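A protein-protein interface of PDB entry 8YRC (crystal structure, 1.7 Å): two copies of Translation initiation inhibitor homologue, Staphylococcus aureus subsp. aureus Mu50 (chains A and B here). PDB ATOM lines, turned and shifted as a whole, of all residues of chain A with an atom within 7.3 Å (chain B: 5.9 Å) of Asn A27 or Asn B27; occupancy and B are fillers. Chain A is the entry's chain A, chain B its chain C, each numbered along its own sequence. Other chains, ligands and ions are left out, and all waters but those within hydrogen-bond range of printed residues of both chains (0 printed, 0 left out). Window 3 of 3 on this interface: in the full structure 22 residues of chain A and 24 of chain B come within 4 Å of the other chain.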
ATOM      1  N   SER A   4      33.077 -26.393   8.490  1.00  0.00           N
ATOM      2  CA  SER A   4      31.793 -25.633   8.362  1.00  0.00           C
ATOM      3  C   SER A   4      30.869 -26.368   7.385  1.00  0.00           C
ATOM      4  O   SER A   4      29.871 -26.950   7.841  1.00  0.00           O
ATOM      5  CB  SER A   4      32.028 -24.209   7.918  1.00  0.00           C
ATOM      6  OG  SER A   4      32.069 -23.335   9.038  1.00  0.00           O
ATOM      7  N   MET A   5      31.211 -26.356   6.096  1.00  0.00           N
ATOM      8  CA  MET A   5      30.481 -27.158   5.085  1.00  0.00           C
ATOM      9  C   MET A   5      31.413 -28.134   4.374  1.00  0.00           C
ATOM     10  O   MET A   5      32.471 -27.706   3.948  1.00  0.00           O
ATOM     11  CB  MET A   5      29.790 -26.305   4.027  1.00  0.00           C
ATOM     12  CG  MET A   5      28.897 -27.215   3.210  1.00  0.00           C
ATOM     13  SD  MET A   5      27.892 -26.392   2.013  1.00  0.00           S
ATOM     14  CE  MET A   5      27.065 -25.200   3.068  1.00  0.00           C
ATOM     15  N   LYS A   6      30.981 -29.385   4.202  1.00  0.00           N
ATOM     16  CA  LYS A   6      31.682 -30.398   3.374  1.00  0.00           C
ATOM     17  C   LYS A   6      30.869 -30.647   2.099  1.00  0.00           C
ATOM     18  O   LYS A   6      29.622 -30.700   2.214  1.00  0.00           O
ATOM     19  CB  LYS A   6      31.792 -31.726   4.118  1.00  0.00           C
ATOM     20  CG  LYS A   6      33.207 -32.208   4.406  1.00  0.00           C
ATOM     21  CD  LYS A   6      33.414 -33.720   4.310  1.00  0.00           C
ATOM     22  CE  LYS A   6      33.487 -34.427   5.647  1.00  0.00           C
ATOM     23  NZ  LYS A   6      33.778 -35.870   5.475  1.00  0.00           N
ATOM     24  N   VAL A  25      27.327 -31.538   3.771  1.00  0.00           N
ATOM     25  CA  VAL A  25      27.251 -31.823   5.227  1.00  0.00           C
ATOM     26  C   VAL A  25      27.472 -30.488   5.917  1.00  0.00           C
ATOM     27  O   VAL A  25      28.507 -29.855   5.620  1.00  0.00           O
ATOM     28  CB  VAL A  25      28.262 -32.895   5.687  1.00  0.00           C
ATOM     29  CG1 VAL A  25      28.061 -33.171   7.163  1.00  0.00           C
ATOM     30  CG2 VAL A  25      28.187 -34.188   4.872  1.00  0.00           C
ATOM     31  N   VAL A  26      26.482 -30.001   6.669  1.00  0.00           N
ATOM     32  CA  VAL A  26      26.509 -28.688   7.375  1.00  0.00           C
ATOM     33  C   VAL A  26      25.900 -28.923   8.758  1.00  0.00           C
ATOM     34  O   VAL A  26      24.851 -29.579   8.823  1.00  0.00           O
ATOM     35  CB  VAL A  26      25.663 -27.585   6.731  1.00  0.00           C
ATOM     36  CG1 VAL A  26      26.257 -26.220   7.036  1.00  0.00           C
ATOM     37  CG2 VAL A  26      25.427 -27.771   5.248  1.00  0.00           C
ATOM     38  N   ASN A  27      26.542 -28.458   9.832  1.00  0.00           N
ATOM     39  CA  ASN A  27      25.903 -28.443  11.178  1.00  0.00           C
ATOM     40  C   ASN A  27      25.408 -29.854  11.536  1.00  0.00           C
ATOM     41  O   ASN A  27      24.334 -29.979  12.107  1.00  0.00           O
ATOM     42  CB  ASN A  27      24.784 -27.397  11.197  1.00  0.00           C
ATOM     43  CG  ASN A  27      25.327 -25.985  11.101  1.00  0.00           C
ATOM     44  OD1 ASN A  27      26.491 -25.775  10.771  1.00  0.00           O
ATOM     45  ND2 ASN A  27      24.489 -24.997  11.363  1.00  0.00           N
ATOM     46  N   GLY A  28      26.192 -30.876  11.193  1.00  0.00           N
ATOM     47  CA  GLY A  28      26.034 -32.277  11.625  1.00  0.00           C
ATOM     48  C   GLY A  28      24.924 -32.996  10.885  1.00  0.00           C
ATOM     49  O   GLY A  28      24.539 -34.108  11.315  1.00  0.00           O
ATOM     50  N   MET A  29      24.457 -32.371   9.798  1.00  0.00           N
ATOM     51  CA  MET A  29      23.359 -32.891   8.947  1.00  0.00           C
ATOM     52  C   MET A  29      23.882 -33.102   7.527  1.00  0.00           C
ATOM     53  O   MET A  29      24.560 -32.181   6.994  1.00  0.00           O
ATOM     54  CB  MET A  29      22.164 -31.940   8.908  1.00  0.00           C
ATOM     55  CG  MET A  29      21.508 -31.711  10.265  1.00  0.00           C
ATOM     56  SD  MET A  29      21.044 -33.235  11.114  1.00  0.00           S
ATOM     57  CE  MET A  29      19.825 -33.989  10.030  1.00  0.00           C
ATOM     58  N   VAL A  30      23.500 -34.231   6.949  1.00  0.00           N
ATOM     59  CA  VAL A  30      23.691 -34.511   5.507  1.00  0.00           C
ATOM     60  C   VAL A  30      22.417 -34.144   4.714  1.00  0.00           C
ATOM     61  O   VAL A  30      21.370 -34.650   5.037  1.00  0.00           O
ATOM     62  CB  VAL A  30      24.038 -35.977   5.249  1.00  0.00           C
ATOM     63  CG1 VAL A  30      24.379 -36.177   3.790  1.00  0.00           C
ATOM     64  CG2 VAL A  30      25.197 -36.442   6.103  1.00  0.00           C
ATOM     65  N   TYR A  31      22.608 -33.458   3.604  1.00  0.00           N
ATOM     66  CA  TYR A  31      21.534 -33.105   2.639  1.00  0.00           C
ATOM     67  C   TYR A  31      21.922 -33.784   1.329  1.00  0.00           C
ATOM     68  O   TYR A  31      22.904 -33.338   0.756  1.00  0.00           O
ATOM     69  CB  TYR A  31      21.412 -31.608   2.454  1.00  0.00           C
ATOM     70  CG  TYR A  31      21.066 -30.854   3.713  1.00  0.00           C
ATOM     71  CD1 TYR A  31      22.042 -30.466   4.628  1.00  0.00           C
ATOM     72  CD2 TYR A  31      19.761 -30.606   4.057  1.00  0.00           C
ATOM     73  CE1 TYR A  31      21.734 -29.788   5.799  1.00  0.00           C
ATOM     74  CE2 TYR A  31      19.438 -29.951   5.236  1.00  0.00           C
ATOM     75  CZ  TYR A  31      20.412 -29.562   6.131  1.00  0.00           C
ATOM     76  OH  TYR A  31      20.071 -28.910   7.296  1.00  0.00           O
ATOM     77  N   LYS A 126      21.429 -37.455   9.873  1.00  0.00           N
ATOM     78  CA  LYS A 126      22.375 -37.043  10.939  1.00  0.00           C
ATOM     79  C   LYS A 126      23.746 -37.701  10.693  1.00  0.00           C
ATOM     80  O   LYS A 126      23.779 -38.876  10.328  1.00  0.00           O
ATOM     81  CB  LYS A 126      21.838 -37.523  12.298  1.00  0.00           C
ATOM     82  CG  LYS A 126      22.521 -36.855  13.480  1.00  0.00           C
ATOM     83  CD  LYS A 126      22.325 -37.527  14.810  1.00  0.00           C
ATOM     84  CE  LYS A 126      23.106 -36.793  15.885  1.00  0.00           C
ATOM     85  NZ  LYS A 126      22.890 -37.382  17.228  1.00  0.00           N
ATOM     86  N   ILE A 127      24.830 -36.949  10.861  1.00  0.00           N
ATOM     87  CA  ILE A 127      26.208 -37.520  10.955  1.00  0.00           C
ATOM     88  C   ILE A 127      26.221 -38.661  11.991  1.00  0.00           C
ATOM     89  O   ILE A 127      25.606 -38.469  13.058  1.00  0.00           O
ATOM     90  CB  ILE A 127      27.182 -36.381  11.337  1.00  0.00           C
ATOM     91  CG1 ILE A 127      27.340 -35.382  10.192  1.00  0.00           C
ATOM     92  CG2 ILE A 127      28.533 -36.901  11.816  1.00  0.00           C
ATOM     93  CD1 ILE A 127      27.618 -36.025   8.873  1.00  0.00           C
ATOM     94  N   VAL B  25      15.444 -18.149  10.009  1.00  0.00           N
ATOM     95  CA  VAL B  25      16.822 -18.562  10.396  1.00  0.00           C
ATOM     96  C   VAL B  25      16.702 -19.226  11.749  1.00  0.00           C
ATOM     97  O   VAL B  25      16.150 -18.556  12.665  1.00  0.00           O
ATOM     98  CB  VAL B  25      17.774 -17.364  10.481  1.00  0.00           C
ATOM     99  CG1 VAL B  25      19.214 -17.800  10.747  1.00  0.00           C
ATOM    100  CG2 VAL B  25      17.671 -16.456   9.275  1.00  0.00           C
ATOM    101  N   VAL B  26      17.124 -20.473  11.833  1.00  0.00           N
ATOM    102  CA  VAL B  26      16.977 -21.339  13.040  1.00  0.00           C
ATOM    103  C   VAL B  26      18.266 -22.140  13.188  1.00  0.00           C
ATOM    104  O   VAL B  26      18.621 -22.810  12.217  1.00  0.00           O
ATOM    105  CB  VAL B  26      15.771 -22.278  12.861  1.00  0.00           C
ATOM    106  CG1 VAL B  26      15.623 -23.242  14.029  1.00  0.00           C
ATOM    107  CG2 VAL B  26      14.489 -21.496  12.631  1.00  0.00           C
ATOM    108  N   ASN B  27      18.941 -22.106  14.340  1.00  0.00           N
ATOM    109  CA  ASN B  27      20.092 -23.026  14.575  1.00  0.00           C
ATOM    110  C   ASN B  27      21.136 -22.872  13.452  1.00  0.00           C
ATOM    111  O   ASN B  27      21.718 -23.913  13.005  1.00  0.00           O
ATOM    112  CB  ASN B  27      19.634 -24.481  14.716  1.00  0.00           C
ATOM    113  CG  ASN B  27      18.789 -24.764  15.939  1.00  0.00           C
ATOM    114  OD1 ASN B  27      18.402 -23.862  16.667  1.00  0.00           O
ATOM    115  ND2 ASN B  27      18.472 -26.026  16.163  1.00  0.00           N
ATOM    116  N   GLY B  28      21.402 -21.632  13.027  1.00  0.00           N
ATOM    117  CA  GLY B  28      22.496 -21.287  12.106  1.00  0.00           C
ATOM    118  C   GLY B  28      22.231 -21.793  10.700  1.00  0.00           C
ATOM    119  O   GLY B  28      23.190 -21.881   9.926  1.00  0.00           O
ATOM    120  N   MET B  29      20.949 -22.016  10.379  1.00  0.00           N
ATOM    121  CA  MET B  29      20.467 -22.440   9.032  1.00  0.00           C
ATOM    122  C   MET B  29      19.331 -21.491   8.598  1.00  0.00           C
ATOM    123  O   MET B  29      18.386 -21.235   9.377  1.00  0.00           O
ATOM    124  CB  MET B  29      20.017 -23.905   9.011  1.00  0.00           C
ATOM    125  CG  MET B  29      21.126 -24.896   9.414  1.00  0.00           C
ATOM    126  SD  MET B  29      22.573 -24.931   8.325  1.00  0.00           S
ATOM    127  CE  MET B  29      21.766 -25.576   6.855  1.00  0.00           C
ATOM    128  N   LYS B 126      23.690 -22.133   5.185  1.00  0.00           N
ATOM    129  CA  LYS B 126      24.387 -21.913   6.478  1.00  0.00           C
ATOM    130  C   LYS B 126      24.514 -20.404   6.705  1.00  0.00           C
ATOM    131  O   LYS B 126      24.755 -19.637   5.746  1.00  0.00           O
ATOM    132  CB  LYS B 126      25.747 -22.624   6.455  1.00  0.00           C
ATOM    133  CG  LYS B 126      26.487 -22.707   7.778  1.00  0.00           C
ATOM    134  CD  LYS B 126      27.941 -23.173   7.628  1.00  0.00           C
ATOM    135  CE  LYS B 126      28.833 -22.717   8.766  1.00  0.00           C
ATOM    136  NZ  LYS B 126      28.182 -22.876  10.092  1.00  0.00           N
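The side-chain amide oxygen (OD1) of Asn A27 lies within hydrogen-bond range of the side-chain amino group (NZ) of Lys B126 (3.4 Å).
The side-chain amide nitrogen of Asn A27 sits at hydrogen-bond distance from the side-chain sulfur of Met B29, at 3.6 Å.
The side-chain amide nitrogen of Asn A27 lies within hydrogen-bond range of the backbone carbonyl oxygen of Asn B27 (3.4 Å).
Among the printed residues, merely in contact across the chains: Ser A4 with Lys B126 (3.3 Å), Val A26 with Lys B126 (3.5 Å), Asn A27 with Gly B28 (3.7 Å) and Tyr A31 with Met B29 (3.8 Å).
Asn A27 touches four residues of chain B.
Of the printed residues of chain B, Tyr A31 touches Met B29.
Lys A126 touches none of the printed residues of chain B.
Of chain A, only Asn A27 (3.4 Å) comes within 4 Å of Asn B27.
Of the printed residues of chain A, Lys B126 touches Ser A4 (3.3 Å), Val A26 (3.5 Å) and Asn A27 (3.4 Å).
The nearest printed residue of chain B that does not touch Asn A27 is Val B26 (6.3 Å).
The nearest printed residue of chain A that does not touch Asn B27 is Val A26 (7.7 Å).
The nearest printed residue of chain B that does not touch Tyr A31 is Asn B27 (7.8 Å).
Of the 12 printed residues of chain A, 4 touch a printed residue of chain B.
Hydrophobic or aromatic side chains of chain A that line the printed part of chain B: Val A26 and Tyr A31.
Hydrophobic or aromatic side chains of chain B that line the printed part of chain A: Met B29.
Among the printed residues, 7 pairs touch across the chains.
Among the printed residues, no Asp or Glu carboxylate lies within 4 Å of a Lys or Arg side-chain nitrogen of the other chain.
Val A26 touches Lys B126, but with the chains exchanged Lys A126 does not touch Val B26 (14.6 Å).
Asn B27 touches its own counterpart, Asn A27.
Asn A27 touches Met B29, but with the chains exchanged Met A29 does not touch Asn B27 (8.3 Å).
Asn A27 touches Lys B126, but with the chains exchanged Lys A126 does not touch Asn B27 (11.7 Å).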
